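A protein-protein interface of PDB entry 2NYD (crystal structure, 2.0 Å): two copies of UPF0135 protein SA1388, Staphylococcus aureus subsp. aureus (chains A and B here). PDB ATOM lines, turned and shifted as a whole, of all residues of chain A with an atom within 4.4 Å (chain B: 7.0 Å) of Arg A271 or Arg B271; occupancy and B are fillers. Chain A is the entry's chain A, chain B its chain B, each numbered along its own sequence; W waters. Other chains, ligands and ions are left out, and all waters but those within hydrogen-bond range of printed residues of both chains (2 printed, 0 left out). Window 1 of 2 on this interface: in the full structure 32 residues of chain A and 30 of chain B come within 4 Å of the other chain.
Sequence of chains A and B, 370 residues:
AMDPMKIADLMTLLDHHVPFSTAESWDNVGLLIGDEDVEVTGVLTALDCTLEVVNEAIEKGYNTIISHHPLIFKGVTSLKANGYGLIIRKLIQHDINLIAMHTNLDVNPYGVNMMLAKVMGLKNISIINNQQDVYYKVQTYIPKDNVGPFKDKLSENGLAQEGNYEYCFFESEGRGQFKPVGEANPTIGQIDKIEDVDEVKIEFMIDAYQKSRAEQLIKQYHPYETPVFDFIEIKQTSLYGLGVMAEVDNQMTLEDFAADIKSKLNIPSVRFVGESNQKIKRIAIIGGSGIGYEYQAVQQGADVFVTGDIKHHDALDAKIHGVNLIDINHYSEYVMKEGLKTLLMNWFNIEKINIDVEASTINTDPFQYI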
ATOM      1  N   VAL A 270      -7.477 -23.865  -6.982  1.00  0.00           N
ATOM      2  CA  VAL A 270      -8.244 -22.633  -7.218  1.00  0.00           C
ATOM      3  C   VAL A 270      -9.205 -22.426  -6.036  1.00  0.00           C
ATOM      4  O   VAL A 270      -9.614 -23.395  -5.346  1.00  0.00           O
ATOM      5  CB  VAL A 270      -8.965 -22.772  -8.600  1.00  0.00           C
ATOM      6  CG1 VAL A 270     -10.175 -21.901  -8.790  1.00  0.00           C
ATOM      7  CG2 VAL A 270      -7.947 -22.587  -9.717  1.00  0.00           C
ATOM      8  N   ARG A 271      -9.575 -21.185  -5.791  1.00  0.00           N
ATOM      9  CA  ARG A 271     -10.566 -20.861  -4.744  1.00  0.00           C
ATOM     10  C   ARG A 271     -11.558 -19.841  -5.263  1.00  0.00           C
ATOM     11  O   ARG A 271     -11.194 -18.988  -6.051  1.00  0.00           O
ATOM     12  CB  ARG A 271      -9.932 -20.369  -3.418  1.00  0.00           C
ATOM     13  CG  ARG A 271      -9.019 -19.141  -3.567  1.00  0.00           C
ATOM     14  CD  ARG A 271      -8.102 -19.050  -2.357  1.00  0.00           C
ATOM     15  NE  ARG A 271      -7.162 -17.953  -2.478  1.00  0.00           N
ATOM     16  CZ  ARG A 271      -6.267 -17.649  -1.544  1.00  0.00           C
ATOM     17  NH1 ARG A 271      -6.175 -18.387  -0.451  1.00  0.00           N
ATOM     18  NH2 ARG A 271      -5.412 -16.649  -1.731  1.00  0.00           N
ATOM     19  N   PHE A 272     -12.835 -19.959  -4.857  1.00  0.00           N
ATOM     20  CA  PHE A 272     -13.833 -19.029  -5.334  1.00  0.00           C
ATOM     21  C   PHE A 272     -14.674 -18.469  -4.187  1.00  0.00           C
ATOM     22  O   PHE A 272     -14.743 -19.033  -3.099  1.00  0.00           O
ATOM     23  CB  PHE A 272     -14.725 -19.599  -6.473  1.00  0.00           C
ATOM     24  CG  PHE A 272     -15.585 -20.785  -6.062  1.00  0.00           C
ATOM     25  CD1 PHE A 272     -16.883 -20.617  -5.572  1.00  0.00           C
ATOM     26  CD2 PHE A 272     -15.090 -22.084  -6.186  1.00  0.00           C
ATOM     27  CE1 PHE A 272     -17.652 -21.745  -5.212  1.00  0.00           C
ATOM     28  CE2 PHE A 272     -15.850 -23.208  -5.843  1.00  0.00           C
ATOM     29  CZ  PHE A 272     -17.121 -23.055  -5.385  1.00  0.00           C
ATOM     30  N   ILE A 310      -5.905 -12.956  -4.140  1.00  0.00           N
ATOM     31  CA  ILE A 310      -7.056 -12.453  -3.388  1.00  0.00           C
ATOM     32  C   ILE A 310      -6.829 -12.732  -1.911  1.00  0.00           C
ATOM     33  O   ILE A 310      -6.468 -13.848  -1.551  1.00  0.00           O
ATOM     34  CB  ILE A 310      -8.383 -13.069  -3.860  1.00  0.00           C
ATOM     35  CG1 ILE A 310      -8.518 -12.903  -5.392  1.00  0.00           C
ATOM     36  CG2 ILE A 310      -9.591 -12.380  -3.108  1.00  0.00           C
ATOM     37  CD1 ILE A 310      -9.821 -13.469  -5.957  1.00  0.00           C
ATOM     38  N   ILE A 326     -13.085 -15.401  -8.396  1.00  0.00           N
ATOM     39  CA  ILE A 326     -12.278 -16.609  -8.473  1.00  0.00           C
ATOM     40  C   ILE A 326     -10.832 -16.164  -8.405  1.00  0.00           C
ATOM     41  O   ILE A 326     -10.425 -15.257  -9.134  1.00  0.00           O
ATOM     42  CB  ILE A 326     -12.514 -17.439  -9.790  1.00  0.00           C
ATOM     43  CG1 ILE A 326     -13.989 -17.911  -9.911  1.00  0.00           C
ATOM     44  CG2 ILE A 326     -11.518 -18.624  -9.860  1.00  0.00           C
ATOM     45  CD1 ILE A 326     -14.351 -18.491 -11.347  1.00  0.00           C
ATOM     46  N   ASP A 327     -10.085 -16.790  -7.496  1.00  0.00           N
ATOM     47  CA  ASP A 327      -8.643 -16.607  -7.401  1.00  0.00           C
ATOM     48  C   ASP A 327      -7.999 -17.758  -8.204  1.00  0.00           C
ATOM     49  O   ASP A 327      -7.962 -18.910  -7.755  1.00  0.00           O
ATOM     50  CB  ASP A 327      -8.182 -16.603  -5.921  1.00  0.00           C
ATOM     51  CG  ASP A 327      -6.715 -16.197  -5.743  1.00  0.00           C
ATOM     52  OD1 ASP A 327      -5.986 -16.096  -6.748  1.00  0.00           O
ATOM     53  OD2 ASP A 327      -6.272 -16.019  -4.592  1.00  0.00           O
ATOM     54  N   ASN A 329      -4.813 -17.509  -8.940  1.00  0.00           N
ATOM     55  CA  ASN A 329      -3.423 -17.242  -8.570  1.00  0.00           C
ATOM     56  C   ASN A 329      -2.769 -16.275  -9.558  1.00  0.00           C
ATOM     57  O   ASN A 329      -2.965 -16.365 -10.764  1.00  0.00           O
ATOM     58  CB  ASN A 329      -2.628 -18.541  -8.357  1.00  0.00           C
ATOM     59  CG  ASN A 329      -3.368 -19.505  -7.425  1.00  0.00           C
ATOM     60  OD1 ASN A 329      -3.820 -19.109  -6.360  1.00  0.00           O
ATOM     61  ND2 ASN A 329      -3.530 -20.749  -7.845  1.00  0.00           N
ATOM     62  N   PHE A 367       5.460 -20.782  -5.121  1.00  0.00           N
ATOM     63  CA  PHE A 367       4.581 -21.636  -4.344  1.00  0.00           C
ATOM     64  C   PHE A 367       4.592 -23.054  -4.838  1.00  0.00           C
ATOM     65  O   PHE A 367       4.491 -23.324  -6.047  1.00  0.00           O
ATOM     66  CB  PHE A 367       3.111 -21.158  -4.369  1.00  0.00           C
ATOM     67  CG  PHE A 367       2.838 -19.907  -3.584  1.00  0.00           C
ATOM     68  CD1 PHE A 367       2.171 -18.826  -4.192  1.00  0.00           C
ATOM     69  CD2 PHE A 367       3.159 -19.831  -2.234  1.00  0.00           C
ATOM     70  CE1 PHE A 367       1.859 -17.649  -3.501  1.00  0.00           C
ATOM     71  CE2 PHE A 367       2.870 -18.646  -1.499  1.00  0.00           C
ATOM     72  CZ  PHE A 367       2.195 -17.553  -2.144  1.00  0.00           C
ATOM     73  N   GLN A 368       4.663 -23.967  -3.866  1.00  0.00           N
ATOM     74  CA  GLN A 368       4.360 -25.371  -4.082  1.00  0.00           C
ATOM     75  C   GLN A 368       3.110 -25.738  -3.237  1.00  0.00           C
ATOM     76  O   GLN A 368       3.034 -25.439  -2.051  1.00  0.00           O
ATOM     77  CB  GLN A 368       5.589 -26.232  -3.684  1.00  0.00           C
ATOM     78  CG  GLN A 368       5.276 -27.704  -3.849  1.00  0.00           C
ATOM     79  CD  GLN A 368       6.516 -28.585  -3.859  1.00  0.00           C
ATOM     80  OE1 GLN A 368       7.641 -28.101  -3.988  1.00  0.00           O
ATOM     81  NE2 GLN A 368       6.302 -29.897  -3.730  1.00  0.00           N
ATOM     82  N   TYR A 369       2.152 -26.410  -3.856  1.00  0.00           N
ATOM     83  CA  TYR A 369       0.835 -26.629  -3.280  1.00  0.00           C
ATOM     84  C   TYR A 369       0.700 -28.047  -2.790  1.00  0.00           C
ATOM     85  O   TYR A 369       1.160 -28.980  -3.449  1.00  0.00           O
ATOM     86  CB  TYR A 369      -0.248 -26.400  -4.342  1.00  0.00           C
ATOM     87  CG  TYR A 369      -0.444 -24.944  -4.641  1.00  0.00           C
ATOM     88  CD1 TYR A 369       0.384 -24.275  -5.551  1.00  0.00           C
ATOM     89  CD2 TYR A 369      -1.486 -24.240  -4.048  1.00  0.00           C
ATOM     90  CE1 TYR A 369       0.177 -22.868  -5.852  1.00  0.00           C
ATOM     91  CE2 TYR A 369      -1.703 -22.863  -4.332  1.00  0.00           C
ATOM     92  CZ  TYR A 369      -0.842 -22.177  -5.183  1.00  0.00           C
ATOM     93  OH  TYR A 369      -1.073 -20.810  -5.411  1.00  0.00           O
ATOM     94  N   ALA B 258       4.513 -28.719   6.399  1.00  0.00           N
ATOM     95  CA  ALA B 258       3.328 -28.213   5.704  1.00  0.00           C
ATOM     96  C   ALA B 258       2.123 -29.188   5.660  1.00  0.00           C
ATOM     97  O   ALA B 258       0.986 -28.775   5.919  1.00  0.00           O
ATOM     98  CB  ALA B 258       3.686 -27.717   4.302  1.00  0.00           C
ATOM     99  N   SER B 269      -6.294 -26.407   1.428  1.00  0.00           N
ATOM    100  CA  SER B 269      -5.137 -26.251   0.546  1.00  0.00           C
ATOM    101  C   SER B 269      -4.108 -25.440   1.322  1.00  0.00           C
ATOM    102  O   SER B 269      -4.461 -24.439   1.913  1.00  0.00           O
ATOM    103  CB  SER B 269      -5.525 -25.456  -0.717  1.00  0.00           C
ATOM    104  OG  SER B 269      -4.390 -25.169  -1.534  1.00  0.00           O
ATOM    105  N   VAL B 270      -2.845 -25.911   1.311  1.00  0.00           N
ATOM    106  CA  VAL B 270      -1.702 -25.200   1.850  1.00  0.00           C
ATOM    107  C   VAL B 270      -0.682 -25.017   0.716  1.00  0.00           C
ATOM    108  O   VAL B 270      -0.645 -25.822  -0.216  1.00  0.00           O
ATOM    109  CB  VAL B 270      -1.151 -25.977   3.098  1.00  0.00           C
ATOM    110  CG1 VAL B 270       0.233 -25.565   3.476  1.00  0.00           C
ATOM    111  CG2 VAL B 270      -2.135 -25.738   4.288  1.00  0.00           C
ATOM    112  N   ARG B 271       0.095 -23.927   0.759  1.00  0.00           N
ATOM    113  CA  ARG B 271       1.219 -23.735  -0.188  1.00  0.00           C
ATOM    114  C   ARG B 271       2.474 -23.279   0.586  1.00  0.00           C
ATOM    115  O   ARG B 271       2.376 -22.578   1.620  1.00  0.00           O
ATOM    116  CB  ARG B 271       0.853 -22.745  -1.325  1.00  0.00           C
ATOM    117  CG  ARG B 271       0.356 -21.382  -0.840  1.00  0.00           C
ATOM    118  CD  ARG B 271      -0.337 -20.616  -1.961  1.00  0.00           C
ATOM    119  NE  ARG B 271      -0.894 -19.355  -1.453  1.00  0.00           N
ATOM    120  CZ  ARG B 271      -1.661 -18.532  -2.156  1.00  0.00           C
ATOM    121  NH1 ARG B 271      -1.935 -18.806  -3.431  1.00  0.00           N
ATOM    122  NH2 ARG B 271      -2.102 -17.390  -1.598  1.00  0.00           N
ATOM    123  N   PHE B 272       3.657 -23.713   0.126  1.00  0.00           N
ATOM    124  CA  PHE B 272       4.851 -23.369   0.843  1.00  0.00           C
ATOM    125  C   PHE B 272       5.887 -22.838  -0.119  1.00  0.00           C
ATOM    126  O   PHE B 272       5.778 -23.018  -1.302  1.00  0.00           O
ATOM    127  CB  PHE B 272       5.386 -24.525   1.708  1.00  0.00           C
ATOM    128  CG  PHE B 272       5.806 -25.759   0.926  1.00  0.00           C
ATOM    129  CD1 PHE B 272       7.097 -25.882   0.426  1.00  0.00           C
ATOM    130  CD2 PHE B 272       4.917 -26.809   0.752  1.00  0.00           C
ATOM    131  CE1 PHE B 272       7.466 -27.038  -0.281  1.00  0.00           C
ATOM    132  CE2 PHE B 272       5.281 -27.973   0.073  1.00  0.00           C
ATOM    133  CZ  PHE B 272       6.566 -28.078  -0.434  1.00  0.00           C
ATOM    134  N   VAL B 273       6.836 -22.090   0.413  1.00  0.00           N
ATOM    135  CA  VAL B 273       7.896 -21.526  -0.392  1.00  0.00           C
ATOM    136  C   VAL B 273       9.169 -22.031   0.222  1.00  0.00           C
ATOM    137  O   VAL B 273       9.435 -21.794   1.403  1.00  0.00           O
ATOM    138  CB  VAL B 273       7.890 -19.966  -0.401  1.00  0.00           C
ATOM    139  CG1 VAL B 273       9.080 -19.388  -1.255  1.00  0.00           C
ATOM    140  CG2 VAL B 273       6.572 -19.458  -0.963  1.00  0.00           C
ATOM    141  N   THR B 307       2.168 -18.053   8.015  1.00  0.00           N
ATOM    142  CA  THR B 307       1.199 -16.940   8.016  1.00  0.00           C
ATOM    143  C   THR B 307       0.101 -17.196   6.990  1.00  0.00           C
ATOM    144  O   THR B 307      -0.001 -18.295   6.467  1.00  0.00           O
ATOM    145  CB  THR B 307       1.894 -15.533   7.824  1.00  0.00           C
ATOM    146  OG1 THR B 307       1.016 -14.477   8.257  1.00  0.00           O
ATOM    147  CG2 THR B 307       2.342 -15.263   6.363  1.00  0.00           C
ATOM    148  N   GLY B 308      -0.748 -16.205   6.717  1.00  0.00           N
ATOM    149  CA  GLY B 308      -1.711 -16.357   5.600  1.00  0.00           C
ATOM    150  C   GLY B 308      -1.620 -15.208   4.642  1.00  0.00           C
ATOM    151  O   GLY B 308      -0.792 -14.324   4.849  1.00  0.00           O
ATOM    152  N   ASP B 309      -2.481 -15.215   3.605  1.00  0.00           N
ATOM    153  CA  ASP B 309      -2.596 -14.152   2.584  1.00  0.00           C
ATOM    154  C   ASP B 309      -1.235 -13.850   1.937  1.00  0.00           C
ATOM    155  O   ASP B 309      -0.935 -12.690   1.662  1.00  0.00           O
ATOM    156  CB  ASP B 309      -3.118 -12.827   3.187  1.00  0.00           C
ATOM    157  CG  ASP B 309      -4.630 -12.800   3.411  1.00  0.00           C
ATOM    158  OD1 ASP B 309      -5.386 -13.637   2.898  1.00  0.00           O
ATOM    159  OD2 ASP B 309      -5.052 -11.867   4.112  1.00  0.00           O
ATOM    160  N   ILE B 310      -0.426 -14.879   1.669  1.00  0.00           N
ATOM    161  CA  ILE B 310       0.853 -14.628   0.986  1.00  0.00           C
ATOM    162  C   ILE B 310       0.631 -14.404  -0.510  1.00  0.00           C
ATOM    163  O   ILE B 310      -0.083 -15.164  -1.147  1.00  0.00           O
ATOM    164  CB  ILE B 310       1.903 -15.739   1.225  1.00  0.00           C
ATOM    165  CG1 ILE B 310       1.989 -16.043   2.760  1.00  0.00           C
ATOM    166  CG2 ILE B 310       3.221 -15.277   0.591  1.00  0.00           C
ATOM    167  CD1 ILE B 310       3.040 -17.139   3.204  1.00  0.00           C
ATOM    168  N   LYS B 311       1.210 -13.325  -1.031  1.00  0.00           N
ATOM    169  CA  LYS B 311       1.076 -12.961  -2.436  1.00  0.00           C
ATOM    170  C   LYS B 311       2.331 -13.303  -3.263  1.00  0.00           C
ATOM    171  O   LYS B 311       3.439 -13.438  -2.728  1.00  0.00           O
ATOM    172  CB  LYS B 311       0.763 -11.476  -2.556  1.00  0.00           C
ATOM    173  CG  LYS B 311      -0.622 -11.127  -1.976  1.00  0.00           C
ATOM    174  CD  LYS B 311      -0.951  -9.639  -2.168  1.00  0.00           C
ATOM    175  CE  LYS B 311       0.083  -8.746  -1.508  1.00  0.00           C
ATOM    176  NZ  LYS B 311      -0.300  -7.271  -1.717  1.00  0.00           N
ATOM    177  N   HIS B 312       2.127 -13.463  -4.566  1.00  0.00           N
ATOM    178  CA  HIS B 312       3.194 -13.873  -5.491  1.00  0.00           C
ATOM    179  C   HIS B 312       4.537 -13.174  -5.288  1.00  0.00           C
ATOM    180  O   HIS B 312       5.552 -13.816  -5.118  1.00  0.00           O
ATOM    181  CB  HIS B 312       2.708 -13.656  -6.939  1.00  0.00           C
ATOM    182  CG  HIS B 312       3.737 -13.968  -7.986  1.00  0.00           C
ATOM    183  ND1 HIS B 312       4.077 -15.257  -8.338  1.00  0.00           N
ATOM    184  CD2 HIS B 312       4.511 -13.147  -8.746  1.00  0.00           C
ATOM    185  CE1 HIS B 312       5.007 -15.223  -9.284  1.00  0.00           C
ATOM    186  NE2 HIS B 312       5.296 -13.953  -9.543  1.00  0.00           N
ATOM    187  N   LEU B 325       8.575 -20.140   3.656  1.00  0.00           N
ATOM    188  CA  LEU B 325       7.234 -19.687   4.058  1.00  0.00           C
ATOM    189  C   LEU B 325       6.252 -20.816   3.933  1.00  0.00           C
ATOM    190  O   LEU B 325       6.429 -21.674   3.071  1.00  0.00           O
ATOM    191  CB  LEU B 325       6.744 -18.567   3.149  1.00  0.00           C
ATOM    192  CG  LEU B 325       7.576 -17.295   3.037  1.00  0.00           C
ATOM    193  CD1 LEU B 325       6.950 -16.430   1.901  1.00  0.00           C
ATOM    194  CD2 LEU B 325       7.788 -16.484   4.350  1.00  0.00           C
ATOM    195  N   ILE B 326       5.216 -20.791   4.785  1.00  0.00           N
ATOM    196  CA  ILE B 326       3.997 -21.572   4.584  1.00  0.00           C
ATOM    197  C   ILE B 326       2.814 -20.629   4.750  1.00  0.00           C
ATOM    198  O   ILE B 326       2.671 -19.960   5.760  1.00  0.00           O
ATOM    199  CB  ILE B 326       3.830 -22.803   5.584  1.00  0.00           C
ATOM    200  CG1 ILE B 326       5.042 -23.752   5.513  1.00  0.00           C
ATOM    201  CG2 ILE B 326       2.500 -23.553   5.334  1.00  0.00           C
ATOM    202  CD1 ILE B 326       5.139 -24.713   6.688  1.00  0.00           C
ATOM    203  N   ASP B 327       1.957 -20.626   3.742  1.00  0.00           N
ATOM    204  CA  ASP B 327       0.664 -19.970   3.783  1.00  0.00           C
ATOM    205  C   ASP B 327      -0.364 -21.006   4.275  1.00  0.00           C
ATOM    206  O   ASP B 327      -0.747 -21.898   3.540  1.00  0.00           O
ATOM    207  CB  ASP B 327       0.336 -19.445   2.364  1.00  0.00           C
ATOM    208  CG  ASP B 327      -0.881 -18.542   2.310  1.00  0.00           C
ATOM    209  OD1 ASP B 327      -1.655 -18.475   3.295  1.00  0.00           O
ATOM    210  OD2 ASP B 327      -1.091 -17.920   1.247  1.00  0.00           O
ATOM    211  N   ILE B 328      -0.805 -20.871   5.521  1.00  0.00           N
ATOM    212  CA  ILE B 328      -1.903 -21.696   6.062  1.00  0.00           C
ATOM    213  C   ILE B 328      -3.275 -21.028   5.855  1.00  0.00           C
ATOM    214  O   ILE B 328      -4.310 -21.551   6.338  1.00  0.00           O
ATOM    215  CB  ILE B 328      -1.732 -21.995   7.569  1.00  0.00           C
ATOM    216  CG1 ILE B 328      -1.603 -20.708   8.388  1.00  0.00           C
ATOM    217  CG2 ILE B 328      -0.541 -22.875   7.795  1.00  0.00           C
ATOM    218  CD1 ILE B 328      -1.702 -20.940   9.951  1.00  0.00           C
ATOM    219  N   ASN B 329      -3.275 -19.913   5.111  1.00  0.00           N
ATOM    220  CA  ASN B 329      -4.469 -19.079   4.874  1.00  0.00           C
ATOM    221  C   ASN B 329      -4.825 -18.205   6.085  1.00  0.00           C
ATOM    222  O   ASN B 329      -4.682 -18.615   7.236  1.00  0.00           O
ATOM    223  CB  ASN B 329      -5.667 -19.905   4.361  1.00  0.00           C
ATOM    224  CG  ASN B 329      -5.296 -20.747   3.116  1.00  0.00           C
ATOM    225  OD1 ASN B 329      -4.656 -20.232   2.217  1.00  0.00           O
ATOM    226  ND2 ASN B 329      -5.594 -22.066   3.142  1.00  0.00           N
ATOM    227  N   HIS B 330      -5.246 -16.983   5.811  1.00  0.00           N
ATOM    228  CA  HIS B 330      -5.661 -16.041   6.872  1.00  0.00           C
ATOM    229  C   HIS B 330      -6.773 -16.705   7.680  1.00  0.00           C
ATOM    230  O   HIS B 330      -6.812 -16.579   8.926  1.00  0.00           O
ATOM    231  CB  HIS B 330      -6.171 -14.770   6.194  1.00  0.00           C
ATOM    232  CG  HIS B 330      -6.380 -13.587   7.093  1.00  0.00           C
ATOM    233  ND1 HIS B 330      -6.029 -12.301   6.709  1.00  0.00           N
ATOM    234  CD2 HIS B 330      -6.899 -13.482   8.342  1.00  0.00           C
ATOM    235  CE1 HIS B 330      -6.373 -11.456   7.669  1.00  0.00           C
ATOM    236  NE2 HIS B 330      -6.916 -12.146   8.664  1.00  0.00           N
ATOM    237  N   PRO B 366     -14.807 -16.950   3.345  1.00  0.00           N
ATOM    238  CA  PRO B 366     -15.370 -16.546   2.061  1.00  0.00           C
ATOM    239  C   PRO B 366     -14.921 -17.417   0.876  1.00  0.00           C
ATOM    240  O   PRO B 366     -15.619 -17.515  -0.110  1.00  0.00           O
ATOM    241  CB  PRO B 366     -14.867 -15.085   1.927  1.00  0.00           C
ATOM    242  CG  PRO B 366     -13.612 -15.072   2.653  1.00  0.00           C
ATOM    243  CD  PRO B 366     -13.938 -15.886   3.887  1.00  0.00           C
ATOM    244  N   PHE B 367     -13.756 -18.053   0.998  1.00  0.00           N
ATOM    245  CA  PHE B 367     -13.211 -18.901  -0.016  1.00  0.00           C
ATOM    246  C   PHE B 367     -13.787 -20.324   0.101  1.00  0.00           C
ATOM    247  O   PHE B 367     -13.938 -20.878   1.192  1.00  0.00           O
ATOM    248  CB  PHE B 367     -11.676 -18.964   0.074  1.00  0.00           C
ATOM    249  CG  PHE B 367     -10.961 -17.714  -0.340  1.00  0.00           C
ATOM    250  CD1 PHE B 367      -9.981 -17.169   0.489  1.00  0.00           C
ATOM    251  CD2 PHE B 367     -11.168 -17.143  -1.608  1.00  0.00           C
ATOM    252  CE1 PHE B 367      -9.280 -16.049   0.125  1.00  0.00           C
ATOM    253  CE2 PHE B 367     -10.464 -16.003  -2.005  1.00  0.00           C
ATOM    254  CZ  PHE B 367      -9.492 -15.463  -1.140  1.00  0.00           C
ATOM    255  N   GLN B 368     -14.115 -20.888  -1.056  1.00  0.00           N
ATOM    256  CA  GLN B 368     -14.316 -22.336  -1.236  1.00  0.00           C
ATOM    257  C   GLN B 368     -13.237 -22.855  -2.210  1.00  0.00           C
ATOM    258  O   GLN B 368     -13.028 -22.282  -3.274  1.00  0.00           O
ATOM    259  CB  GLN B 368     -15.735 -22.624  -1.772  1.00  0.00           C
ATOM    260  CG  GLN B 368     -15.978 -24.111  -1.932  1.00  0.00           C
ATOM    261  CD  GLN B 368     -17.421 -24.466  -2.216  1.00  0.00           C
ATOM    262  OE1 GLN B 368     -18.358 -23.677  -1.943  1.00  0.00           O
ATOM    263  NE2 GLN B 368     -17.612 -25.662  -2.819  1.00  0.00           N
ATOM    264  N   TYR B 369     -12.549 -23.917  -1.810  1.00  0.00           N
ATOM    265  CA  TYR B 369     -11.419 -24.465  -2.518  1.00  0.00           C
ATOM    266  C   TYR B 369     -11.821 -25.625  -3.389  1.00  0.00           C
ATOM    267  O   TYR B 369     -12.653 -26.460  -2.976  1.00  0.00           O
ATOM    268  CB  TYR B 369     -10.328 -24.933  -1.555  1.00  0.00           C
ATOM    269  CG  TYR B 369      -9.631 -23.776  -0.886  1.00  0.00           C
ATOM    270  CD1 TYR B 369     -10.245 -23.100   0.190  1.00  0.00           C
ATOM    271  CD2 TYR B 369      -8.389 -23.328  -1.344  1.00  0.00           C
ATOM    272  CE1 TYR B 369      -9.628 -22.038   0.815  1.00  0.00           C
ATOM    273  CE2 TYR B 369      -7.752 -22.235  -0.727  1.00  0.00           C
ATOM    274  CZ  TYR B 369      -8.384 -21.596   0.355  1.00  0.00           C
ATOM    275  OH  TYR B 369      -7.836 -20.493   0.971  1.00  0.00           O
ATOM    276  N   ILE B 370     -11.250 -25.655  -4.587  1.00  0.00           N
ATOM    277  CA  ILE B 370     -11.445 -26.769  -5.512  1.00  0.00           C
ATOM    278  C   ILE B 370     -10.146 -27.234  -6.207  1.00  0.00           C
ATOM    279  O   ILE B 370     -10.168 -28.298  -6.861  1.00  0.00           O
ATOM    280  CB  ILE B 370     -12.622 -26.486  -6.526  1.00  0.00           C
ATOM    281  CG1 ILE B 370     -12.448 -25.196  -7.294  1.00  0.00           C
ATOM    282  CG2 ILE B 370     -13.956 -26.406  -5.798  1.00  0.00           C
ATOM    283  CD1 ILE B 370     -11.899 -25.341  -8.698  1.00  0.00           C
ATOM    284  OXT ILE B 370      -9.079 -26.573  -6.122  1.00  0.00           O
HETATM  285  O   HOH W   1      -3.565 -16.845  -4.804  1.00  0.00           O
HETATM  286  O   HOH W   2      -3.920 -17.615   1.282  1.00  0.00           O
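Of the 10 printed residues of chain A, 8 touch a printed residue of chain B.
Printed residues of chain A that touch a printed residue of chain B: Val A270, Arg A271, Phe A272, Ile A310, Asn A329, Phe A367, Gln A368 and Tyr A369.
Hydrophobic or aromatic side chains of chain A that line the printed part of chain B: Val A270, Phe A272, Ile A310, Phe A367 and Tyr A369.
Hydrophobic or aromatic side chains of chain B that line the printed part of chain A: Phe B272, Val B273, Ile B310, Phe B367, Tyr B369 and Ile B370.
Among the printed residues, 22 pairs touch across the chains.
Among the printed residues, merely in contact across the chains: Gln A368 with Arg B271 (3.1 Å), Arg A271 with Gln B368 (3.2 Å), Phe A272 with Phe B367 (3.4 Å), Phe A367 with Ile B310 (3.4 Å), Ile A310 with Phe B367 (3.5 Å), Phe A367 with Arg B271 (3.5 Å), Tyr A369 with Val B270 (3.5 Å), Val A270 with Tyr B369 (3.5 Å), Arg A271 with Phe B367 (3.5 Å), Phe A367 with Phe B272 (3.5 Å), Arg A271 with Asn B329 (3.6 Å), Phe A367 with Val B273 (3.7 Å), Phe A272 with Ile B370 (3.7 Å) and Tyr A369 with Ser B269 (3.95 Å).
Printed residues of chain B within 4 Å of Val A270: Tyr B369 (3.5 Å) and Ile B370 (2.9 Å).
Arg A271 touches five residues of chain B.
Printed residues of chain B within 4 Å of Phe A272: Pro B366, Phe B367, Gln B368 and Ile B370.
Asp B327 touches none of the printed residues of chain A.
Of the printed residues of chain A, Pro B366 touches Phe A272.
Of the printed residues of chain A, Phe B367 touches Arg A271 (3.5 Å), Phe A272 (3.4 Å) and Ile A310 (3.5 Å).
The nearest printed residue of chain B that does not touch Gln A368 is Val B270 (4.1 Å).
The guanidinium group (NE) of Arg A271 is in salt-bridge range of the side-chain carboxylate (OD2) of Asp A327 (3.0 Å).
OD1 of Asp A327 lies within hydrogen-bond range of N of Asn A329 (2.9 Å).
The backbone carbonyl oxygen (O) of Ile B310 is in hydrogen-bond range of the guanidinium group (NH2) of Arg B271 (3.0 Å).
The guanidinium group (NE) of Arg B271 is in salt-bridge range of the side-chain carboxylate (OD2) of Asp B327 (3.1 Å).
The backbone carbonyl oxygen of Leu B325 lies within hydrogen-bond range of the backbone NH of Val B273.
N of Ile B310 is in hydrogen-bond range of OD2 of Asp B327 (3.1 Å).
Water W1 lies within hydrogen-bond range of OD1 of Asn A329 (2.8 Å), OD2 of Asp A327 (2.8 Å) and NH1 of Arg B271 (2.9 Å).
Water W2 lies within hydrogen-bond range of OD2 of Asp B327, OD1 of Asn B329, NH1 of Arg A271 and NH2 of Arg B271.
The backbone carbonyl oxygen of Val A270 sits at hydrogen-bond distance from the backbone NH of Ile B370, at 2.9 Å.
NH1 of Arg A271 lies within hydrogen-bond range of OH of Tyr B369.
The backbone NH (N) of Phe A272 lies within hydrogen-bond range of the backbone carbonyl oxygen (O) of Gln B368, at 2.8 Å.
The side-chain amide oxygen (OD1) of Asn A329 sits at hydrogen-bond distance from the guanidinium group (NH1) of Arg B271 (3.5 Å).
The backbone carbonyl oxygen (O) of Gln A368 lies within hydrogen-bond range of the backbone NH (N) of Phe B272 (2.8 Å).
The guanidinium group of Arg B271 lies within hydrogen-bond range of the side-chain hydroxyl of Tyr A369.
The guanidinium group (NH2) of Arg A271 sits close to the guanidinium group (NH2) of Arg B271 (3.4 Å).
The backbone carbonyl oxygen (O) of Pro B366 sits close to the backbone carbonyl oxygen (O) of Phe A272, 3.5 Å away.
Val A270 touches Tyr B369, and with the chains exchanged Tyr A369 touches Val B270.
Arg B271 touches its own counterpart, Arg A271.
Arg A271 touches Tyr B369, and with the chains exchanged Tyr A369 touches Arg B271.
Phe A272 touches Phe B367, and with the chains exchanged Phe A367 touches Phe B272.
Positions printed for both chains: 270, 271, 272, 310, 326, 327, 329, 367, 368 and 369.
Of the 22 pairs that touch across the chains among the printed residues, 17 have their exchanged pair printed and touching as well.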
